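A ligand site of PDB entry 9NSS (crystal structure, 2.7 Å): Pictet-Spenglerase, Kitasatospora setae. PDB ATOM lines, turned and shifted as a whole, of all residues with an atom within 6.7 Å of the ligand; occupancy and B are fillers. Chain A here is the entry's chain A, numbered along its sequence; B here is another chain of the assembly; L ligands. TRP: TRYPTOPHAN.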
ATOM      1  N   ARG A  52      18.564 -14.399  26.482  1.00  0.00           N
ATOM      2  CA  ARG A  52      20.038 -14.581  26.448  1.00  0.00           C
ATOM      3  C   ARG A  52      20.641 -14.021  27.743  1.00  0.00           C
ATOM      4  O   ARG A  52      21.341 -14.780  28.460  1.00  0.00           O
ATOM      5  CB  ARG A  52      20.622 -13.888  25.215  1.00  0.00           C
ATOM      6  CG  ARG A  52      22.108 -14.129  24.976  1.00  0.00           C
ATOM      7  CD  ARG A  52      22.901 -12.866  25.173  1.00  0.00           C
ATOM      8  NE  ARG A  52      22.849 -11.970  24.013  1.00  0.00           N
ATOM      9  CZ  ARG A  52      22.087 -10.894  23.937  1.00  0.00           C
ATOM     10  NH1 ARG A  52      21.664 -10.303  25.036  1.00  0.00           N
ATOM     11  NH2 ARG A  52      21.741 -10.407  22.751  1.00  0.00           N
ATOM     12  N   ASP A  53      20.373 -12.747  28.044  1.00  0.00           N
ATOM     13  CA  ASP A  53      20.975 -12.102  29.242  1.00  0.00           C
ATOM     14  C   ASP A  53      20.329 -12.681  30.506  1.00  0.00           C
ATOM     15  O   ASP A  53      20.979 -12.652  31.566  1.00  0.00           O
ATOM     16  CB  ASP A  53      20.935 -10.592  29.111  1.00  0.00           C
ATOM     17  CG  ASP A  53      21.705 -10.044  27.913  1.00  0.00           C
ATOM     18  OD1 ASP A  53      22.852 -10.461  27.693  1.00  0.00           O
ATOM     19  OD2 ASP A  53      21.156  -9.228  27.181  1.00  0.00           O
ATOM     20  N   MET A  56      22.464 -15.479  31.390  1.00  0.00           N
ATOM     21  CA  MET A  56      23.692 -14.927  31.999  1.00  0.00           C
ATOM     22  C   MET A  56      23.447 -14.667  33.495  1.00  0.00           C
ATOM     23  O   MET A  56      24.313 -15.040  34.304  1.00  0.00           O
ATOM     24  CB  MET A  56      24.112 -13.618  31.305  1.00  0.00           C
ATOM     25  CG  MET A  56      24.476 -13.782  29.846  1.00  0.00           C
ATOM     26  SD  MET A  56      25.913 -12.779  29.384  1.00  0.00           S
ATOM     27  CE  MET A  56      25.128 -11.167  29.213  1.00  0.00           C
ATOM     28  N   THR A 130      18.086 -20.433  24.810  1.00  0.00           N
ATOM     29  CA  THR A 130      18.954 -19.376  24.270  1.00  0.00           C
ATOM     30  C   THR A 130      19.753 -19.891  23.088  1.00  0.00           C
ATOM     31  O   THR A 130      19.926 -19.154  22.107  1.00  0.00           O
ATOM     32  CB  THR A 130      19.885 -18.908  25.387  1.00  0.00           C
ATOM     33  OG1 THR A 130      19.089 -18.281  26.395  1.00  0.00           O
ATOM     34  CG2 THR A 130      20.936 -17.962  24.873  1.00  0.00           C
ATOM     35  N   HIS A 134      19.552 -18.026  19.496  1.00  0.00           N
ATOM     36  CA  HIS A 134      20.720 -17.523  18.738  1.00  0.00           C
ATOM     37  C   HIS A 134      20.690 -18.114  17.324  1.00  0.00           C
ATOM     38  O   HIS A 134      20.899 -17.400  16.342  1.00  0.00           O
ATOM     39  CB  HIS A 134      22.019 -17.928  19.444  1.00  0.00           C
ATOM     40  CG  HIS A 134      23.221 -17.234  18.896  1.00  0.00           C
ATOM     41  ND1 HIS A 134      23.526 -15.936  19.240  1.00  0.00           N
ATOM     42  CD2 HIS A 134      24.162 -17.621  18.040  1.00  0.00           C
ATOM     43  CE1 HIS A 134      24.621 -15.559  18.606  1.00  0.00           C
ATOM     44  NE2 HIS A 134      25.037 -16.564  17.871  1.00  0.00           N
ATOM     45  N   HIS A 221      27.543 -20.100  15.058  1.00  0.00           N
ATOM     46  CA  HIS A 221      28.698 -19.184  14.889  1.00  0.00           C
ATOM     47  C   HIS A 221      28.644 -18.010  15.845  1.00  0.00           C
ATOM     48  O   HIS A 221      27.542 -17.586  16.250  1.00  0.00           O
ATOM     49  CB  HIS A 221      28.668 -18.639  13.460  1.00  0.00           C
ATOM     50  CG  HIS A 221      30.026 -18.302  12.937  1.00  0.00           C
ATOM     51  ND1 HIS A 221      30.618 -17.083  13.166  1.00  0.00           N
ATOM     52  CD2 HIS A 221      30.912 -19.032  12.255  1.00  0.00           C
ATOM     53  CE1 HIS A 221      31.815 -17.072  12.608  1.00  0.00           C
ATOM     54  NE2 HIS A 221      32.025 -18.249  12.061  1.00  0.00           N
ATOM     55  N   ALA A 222      29.827 -17.499  16.213  1.00  0.00           N
ATOM     56  CA  ALA A 222      29.896 -16.233  16.956  1.00  0.00           C
ATOM     57  C   ALA A 222      29.294 -15.142  16.069  1.00  0.00           C
ATOM     58  O   ALA A 222      29.406 -15.217  14.823  1.00  0.00           O
ATOM     59  CB  ALA A 222      31.348 -15.905  17.274  1.00  0.00           C
ATOM     60  N   VAL A 223      28.667 -14.148  16.694  1.00  0.00           N
ATOM     61  CA  VAL A 223      28.113 -13.026  15.882  1.00  0.00           C
ATOM     62  C   VAL A 223      28.822 -11.704  16.194  1.00  0.00           C
ATOM     63  O   VAL A 223      28.759 -10.804  15.349  1.00  0.00           O
ATOM     64  CB  VAL A 223      26.594 -12.903  16.091  1.00  0.00           C
ATOM     65  CG1 VAL A 223      25.883 -14.026  15.366  1.00  0.00           C
ATOM     66  CG2 VAL A 223      26.237 -12.918  17.571  1.00  0.00           C
ATOM     67  N   VAL A 224      29.482 -11.582  17.345  1.00  0.00           N
ATOM     68  CA  VAL A 224      30.235 -10.336  17.626  1.00  0.00           C
ATOM     69  C   VAL A 224      31.734 -10.596  17.589  1.00  0.00           C
ATOM     70  O   VAL A 224      32.468  -9.709  17.121  1.00  0.00           O
ATOM     71  CB  VAL A 224      29.822  -9.827  19.021  1.00  0.00           C
ATOM     72  CG1 VAL A 224      30.454  -8.481  19.327  1.00  0.00           C
ATOM     73  CG2 VAL A 224      28.316  -9.761  19.179  1.00  0.00           C
ATOM     74  N   SER A 225      32.172 -11.801  17.988  1.00  0.00           N
ATOM     75  CA  SER A 225      33.614 -12.077  18.216  1.00  0.00           C
ATOM     76  C   SER A 225      34.463 -12.181  16.950  1.00  0.00           C
ATOM     77  O   SER A 225      35.662 -11.830  17.020  1.00  0.00           O
ATOM     78  CB  SER A 225      33.750 -13.342  19.045  1.00  0.00           C
ATOM     79  OG  SER A 225      32.712 -13.446  20.022  1.00  0.00           O
ATOM     80  N   GLY A 226      33.926 -12.700  15.856  1.00  0.00           N
ATOM     81  CA  GLY A 226      34.827 -12.849  14.702  1.00  0.00           C
ATOM     82  C   GLY A 226      34.886 -14.276  14.227  1.00  0.00           C
ATOM     83  O   GLY A 226      33.811 -14.896  14.122  1.00  0.00           O
ATOM     84  N   TYR A 230      30.692 -21.751  18.246  1.00  0.00           N
ATOM     85  CA  TYR A 230      30.430 -22.279  19.614  1.00  0.00           C
ATOM     86  C   TYR A 230      29.117 -23.024  19.622  1.00  0.00           C
ATOM     87  O   TYR A 230      28.216 -22.735  18.808  1.00  0.00           O
ATOM     88  CB  TYR A 230      30.438 -21.187  20.671  1.00  0.00           C
ATOM     89  CG  TYR A 230      29.606 -19.954  20.391  1.00  0.00           C
ATOM     90  CD1 TYR A 230      28.230 -20.033  20.204  1.00  0.00           C
ATOM     91  CD2 TYR A 230      30.196 -18.695  20.362  1.00  0.00           C
ATOM     92  CE1 TYR A 230      27.465 -18.884  19.970  1.00  0.00           C
ATOM     93  CE2 TYR A 230      29.451 -17.556  20.139  1.00  0.00           C
ATOM     94  CZ  TYR A 230      28.091 -17.648  19.940  1.00  0.00           C
ATOM     95  OH  TYR A 230      27.367 -16.514  19.719  1.00  0.00           O
ATOM     96  N   TRP A 232      26.213 -24.854  22.487  1.00  0.00           N
ATOM     97  CA  TRP A 232      25.770 -25.030  23.888  1.00  0.00           C
ATOM     98  C   TRP A 232      25.885 -26.489  24.259  1.00  0.00           C
ATOM     99  O   TRP A 232      25.059 -27.319  23.840  1.00  0.00           O
ATOM    100  CB  TRP A 232      24.332 -24.529  24.039  1.00  0.00           C
ATOM    101  CG  TRP A 232      24.234 -23.035  24.174  1.00  0.00           C
ATOM    102  CD1 TRP A 232      23.998 -22.318  25.313  1.00  0.00           C
ATOM    103  CD2 TRP A 232      24.388 -22.080  23.109  1.00  0.00           C
ATOM    104  NE1 TRP A 232      23.987 -20.981  25.035  1.00  0.00           N
ATOM    105  CE2 TRP A 232      24.212 -20.796  23.692  1.00  0.00           C
ATOM    106  CE3 TRP A 232      24.642 -22.174  21.743  1.00  0.00           C
ATOM    107  CZ2 TRP A 232      24.307 -19.635  22.944  1.00  0.00           C
ATOM    108  CZ3 TRP A 232      24.722 -21.009  21.004  1.00  0.00           C
ATOM    109  CH2 TRP A 232      24.560 -19.758  21.599  1.00  0.00           C
ATOM    110  N   ILE A 247      40.983 -14.165  24.009  1.00  0.00           N
ATOM    111  CA  ILE A 247      40.393 -14.651  22.733  1.00  0.00           C
ATOM    112  C   ILE A 247      41.230 -14.145  21.554  1.00  0.00           C
ATOM    113  O   ILE A 247      41.524 -14.946  20.655  1.00  0.00           O
ATOM    114  CB  ILE A 247      38.946 -14.121  22.654  1.00  0.00           C
ATOM    115  CG1 ILE A 247      37.994 -15.018  23.435  1.00  0.00           C
ATOM    116  CG2 ILE A 247      38.516 -13.916  21.193  1.00  0.00           C
ATOM    117  CD1 ILE A 247      36.577 -14.478  23.518  1.00  0.00           C
ATOM    118  N   THR A 261      28.658 -17.221  30.089  1.00  0.00           N
ATOM    119  CA  THR A 261      27.550 -16.872  29.181  1.00  0.00           C
ATOM    120  C   THR A 261      26.828 -18.142  28.800  1.00  0.00           C
ATOM    121  O   THR A 261      26.274 -18.202  27.681  1.00  0.00           O
ATOM    122  CB  THR A 261      28.095 -16.148  27.953  1.00  0.00           C
ATOM    123  OG1 THR A 261      28.599 -17.179  27.105  1.00  0.00           O
ATOM    124  CG2 THR A 261      29.222 -15.188  28.295  1.00  0.00           C
ATOM    125  N   GLY A 262      26.821 -19.132  29.695  1.00  0.00           N
ATOM    126  CA  GLY A 262      26.231 -20.447  29.365  1.00  0.00           C
ATOM    127  C   GLY A 262      27.316 -21.349  28.809  1.00  0.00           C
ATOM    128  O   GLY A 262      28.071 -20.862  27.955  1.00  0.00           O
ATOM    129  N   LYS A 264      29.504 -23.119  26.615  1.00  0.00           N
ATOM    130  CA  LYS A 264      29.550 -23.381  25.156  1.00  0.00           C
ATOM    131  C   LYS A 264      30.950 -23.875  24.750  1.00  0.00           C
ATOM    132  O   LYS A 264      31.944 -23.242  25.149  1.00  0.00           O
ATOM    133  CB  LYS A 264      29.204 -22.110  24.365  1.00  0.00           C
ATOM    134  CG  LYS A 264      27.843 -21.507  24.667  1.00  0.00           C
ATOM    135  CD  LYS A 264      27.265 -20.709  23.500  1.00  0.00           C
ATOM    136  CE  LYS A 264      28.112 -19.537  23.118  1.00  0.00           C
ATOM    137  NZ  LYS A 264      28.721 -18.877  24.279  1.00  0.00           N
ATOM    138  N   GLU A 274      37.639  -9.977  19.908  1.00  0.00           N
ATOM    139  CA  GLU A 274      37.224  -9.932  21.323  1.00  0.00           C
ATOM    140  C   GLU A 274      38.492 -10.008  22.191  1.00  0.00           C
ATOM    141  O   GLU A 274      39.364 -10.853  21.920  1.00  0.00           O
ATOM    142  CB  GLU A 274      36.285 -11.100  21.612  1.00  0.00           C
ATOM    143  CG  GLU A 274      35.719 -11.087  23.029  1.00  0.00           C
ATOM    144  CD  GLU A 274      34.283 -11.561  23.072  1.00  0.00           C
ATOM    145  OE1 GLU A 274      33.573 -11.354  22.068  1.00  0.00           O
ATOM    146  OE2 GLU A 274      33.871 -12.149  24.095  1.00  0.00           O
ATOM    147  N   SER B  36      30.977 -10.018  14.075  1.00  0.00           N
ATOM    148  CA  SER B  36      31.412 -10.986  13.043  1.00  0.00           C
ATOM    149  C   SER B  36      30.736 -10.649  11.703  1.00  0.00           C
ATOM    150  O   SER B  36      29.492 -10.525  11.706  1.00  0.00           O
ATOM    151  CB  SER B  36      31.119 -12.409  13.458  1.00  0.00           C
ATOM    152  OG  SER B  36      31.512 -12.641  14.804  1.00  0.00           O
ATOM    153  N   PHE B  46      23.712  -6.103  19.981  1.00  0.00           N
ATOM    154  CA  PHE B  46      24.178  -6.589  21.267  1.00  0.00           C
ATOM    155  C   PHE B  46      24.357  -5.443  22.236  1.00  0.00           C
ATOM    156  O   PHE B  46      23.880  -5.495  23.362  1.00  0.00           O
ATOM    157  CB  PHE B  46      25.483  -7.347  21.090  1.00  0.00           C
ATOM    158  CG  PHE B  46      25.345  -8.826  21.275  1.00  0.00           C
ATOM    159  CD1 PHE B  46      24.694  -9.578  20.299  1.00  0.00           C
ATOM    160  CD2 PHE B  46      25.847  -9.448  22.407  1.00  0.00           C
ATOM    161  CE1 PHE B  46      24.556 -10.948  20.449  1.00  0.00           C
ATOM    162  CE2 PHE B  46      25.728 -10.827  22.568  1.00  0.00           C
ATOM    163  CZ  PHE B  46      25.077 -11.579  21.592  1.00  0.00           C
ATOM    164  N   ILE B  50      22.124  -5.336  25.594  1.00  0.00           N
ATOM    165  CA  ILE B  50      22.830  -5.671  26.820  1.00  0.00           C
ATOM    166  C   ILE B  50      22.950  -4.468  27.734  1.00  0.00           C
ATOM    167  O   ILE B  50      22.835  -4.626  28.956  1.00  0.00           O
ATOM    168  CB  ILE B  50      24.198  -6.289  26.502  1.00  0.00           C
ATOM    169  CG1 ILE B  50      23.967  -7.586  25.717  1.00  0.00           C
ATOM    170  CG2 ILE B  50      24.980  -6.546  27.784  1.00  0.00           C
ATOM    171  CD1 ILE B  50      25.064  -8.635  25.857  1.00  0.00           C
ATOM    172  N   ILE B  85      30.586  -9.831  33.859  1.00  0.00           N
ATOM    173  CA  ILE B  85      30.148 -10.379  32.567  1.00  0.00           C
ATOM    174  C   ILE B  85      29.448  -9.302  31.742  1.00  0.00           C
ATOM    175  O   ILE B  85      29.562  -9.280  30.501  1.00  0.00           O
ATOM    176  CB  ILE B  85      29.267 -11.649  32.752  1.00  0.00           C
ATOM    177  CG1 ILE B  85      29.071 -12.367  31.421  1.00  0.00           C
ATOM    178  CG2 ILE B  85      27.911 -11.326  33.352  1.00  0.00           C
ATOM    179  CD1 ILE B  85      30.372 -12.733  30.740  1.00  0.00           C
ATOM    180  N   PHE B  89      31.971  -6.868  28.935  1.00  0.00           N
ATOM    181  CA  PHE B  89      31.501  -6.974  27.566  1.00  0.00           C
ATOM    182  C   PHE B  89      31.073  -5.623  27.028  1.00  0.00           C
ATOM    183  O   PHE B  89      31.336  -5.321  25.856  1.00  0.00           O
ATOM    184  CB  PHE B  89      30.327  -7.932  27.443  1.00  0.00           C
ATOM    185  CG  PHE B  89      29.719  -7.913  26.072  1.00  0.00           C
ATOM    186  CD1 PHE B  89      30.362  -8.540  25.003  1.00  0.00           C
ATOM    187  CD2 PHE B  89      28.542  -7.231  25.821  1.00  0.00           C
ATOM    188  CE1 PHE B  89      29.816  -8.510  23.746  1.00  0.00           C
ATOM    189  CE2 PHE B  89      27.995  -7.188  24.558  1.00  0.00           C
ATOM    190  CZ  PHE B  89      28.635  -7.834  23.513  1.00  0.00           C
ATOM    191  N   TYR B  92      33.992  -3.656  25.957  1.00  0.00           N
ATOM    192  CA  TYR B  92      34.430  -4.143  24.651  1.00  0.00           C
ATOM    193  C   TYR B  92      33.547  -3.588  23.538  1.00  0.00           C
ATOM    194  O   TYR B  92      34.046  -3.155  22.495  1.00  0.00           O
ATOM    195  CB  TYR B  92      34.430  -5.681  24.633  1.00  0.00           C
ATOM    196  CG  TYR B  92      34.452  -6.313  23.256  1.00  0.00           C
ATOM    197  CD1 TYR B  92      35.588  -6.222  22.435  1.00  0.00           C
ATOM    198  CD2 TYR B  92      33.341  -7.020  22.753  1.00  0.00           C
ATOM    199  CE1 TYR B  92      35.617  -6.808  21.153  1.00  0.00           C
ATOM    200  CE2 TYR B  92      33.365  -7.613  21.457  1.00  0.00           C
ATOM    201  CZ  TYR B  92      34.518  -7.496  20.670  1.00  0.00           C
ATOM    202  OH  TYR B  92      34.599  -8.052  19.410  1.00  0.00           O
HETATM  203  N   TRP L   1      31.153 -12.459  22.149  1.00  0.00           N
HETATM  204  CA  TRP L   1      29.797 -13.019  21.990  1.00  0.00           C
HETATM  205  C   TRP L   1      29.427 -13.215  20.508  1.00  0.00           C
HETATM  206  O   TRP L   1      30.174 -12.820  19.628  1.00  0.00           O
HETATM  207  CB  TRP L   1      28.789 -12.097  22.678  1.00  0.00           C
HETATM  208  CG  TRP L   1      28.066 -12.726  23.832  1.00  0.00           C
HETATM  209  CD1 TRP L   1      28.133 -12.351  25.139  1.00  0.00           C
HETATM  210  CD2 TRP L   1      27.168 -13.860  23.783  1.00  0.00           C
HETATM  211  NE1 TRP L   1      27.336 -13.157  25.907  1.00  0.00           N
HETATM  212  CE2 TRP L   1      26.733 -14.086  25.113  1.00  0.00           C
HETATM  213  CE3 TRP L   1      26.678 -14.685  22.767  1.00  0.00           C
HETATM  214  CZ2 TRP L   1      25.845 -15.119  25.431  1.00  0.00           C
HETATM  215  CZ3 TRP L   1      25.808 -15.702  23.084  1.00  0.00           C
HETATM  216  CH2 TRP L   1      25.396 -15.918  24.400  1.00  0.00           C
HETATM  217  OXT TRP L   1      28.347 -13.766  20.254  1.00  0.00           O
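The backbone NH (N) of Ser 225 lies within hydrogen-bond range of an oxygen (O) of the ligand (2.8 Å). The side-chain hydroxyl (OG) of Ser 225 lies within hydrogen-bond range of an oxygen (O) of the ligand (2.6 Å). A nitrogen (N) of the ligand lies within salt-bridge range of the side-chain carboxylate (OE1) of Glu 274 (2.7 Å). N of Val 224 lies within hydrogen-bond range of O of the ligand (2.7 Å). An oxygen (OXT) of the ligand sits at hydrogen-bond distance from the side-chain hydroxyl (OH) of Tyr 230, 3.0 Å away. A nitrogen (NE1) of the ligand is in hydrogen-bond range of the side-chain sulfur of Met 56 (3.8 Å).
CD of Arg 52 touches CZ2 of the ligand, 3.7 Å away. Val 223 touches the ligand. Thr 261 touches the ligand. CE2 of Phe 46 of chain B touches CG of the ligand (3.3 Å). CE1 of Phe 89 of chain B touches CB of the ligand (3.9 Å). Hydrophobic or aromatic side chains that line the ligand: Met 56, Val 223, Val 224, Tyr 230, Phe 46 of chain B and Phe 89 of chain B. Within 4 Å of the ligand: Arg 52, Met 56, Val 223, Val 224, Ser 225, Tyr 230, Thr 261, Glu 274, Phe 46 of chain B and Phe 89 of chain B. The nearest printed residue that does not touch the ligand is Ala 222 (4.1 Å).
OG of Ser 225 sits at hydrogen-bond distance from OE1 of Glu 274 (3.1 Å). The backbone NH of Ser 225 is in hydrogen-bond range of the side-chain hydroxyl of Ser 36 of chain B. The backbone NH (N) of Ser 36 of chain B lies within hydrogen-bond range of the backbone carbonyl oxygen (O) of Val 224, 3.4 Å away. A ring nitrogen (NE2) of His 134 sits at hydrogen-bond distance from the side-chain hydroxyl (OH) of Tyr 230 (3.0 Å). O of Val 223 is in hydrogen-bond range of N of Ser 36 of chain B (2.7 Å). OG1 of Thr 261 lies within hydrogen-bond range of NZ of Lys 264. The guanidinium group of Arg 52 lies within salt-bridge range of the side-chain carboxylate of Asp 53 (2.5 Å).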
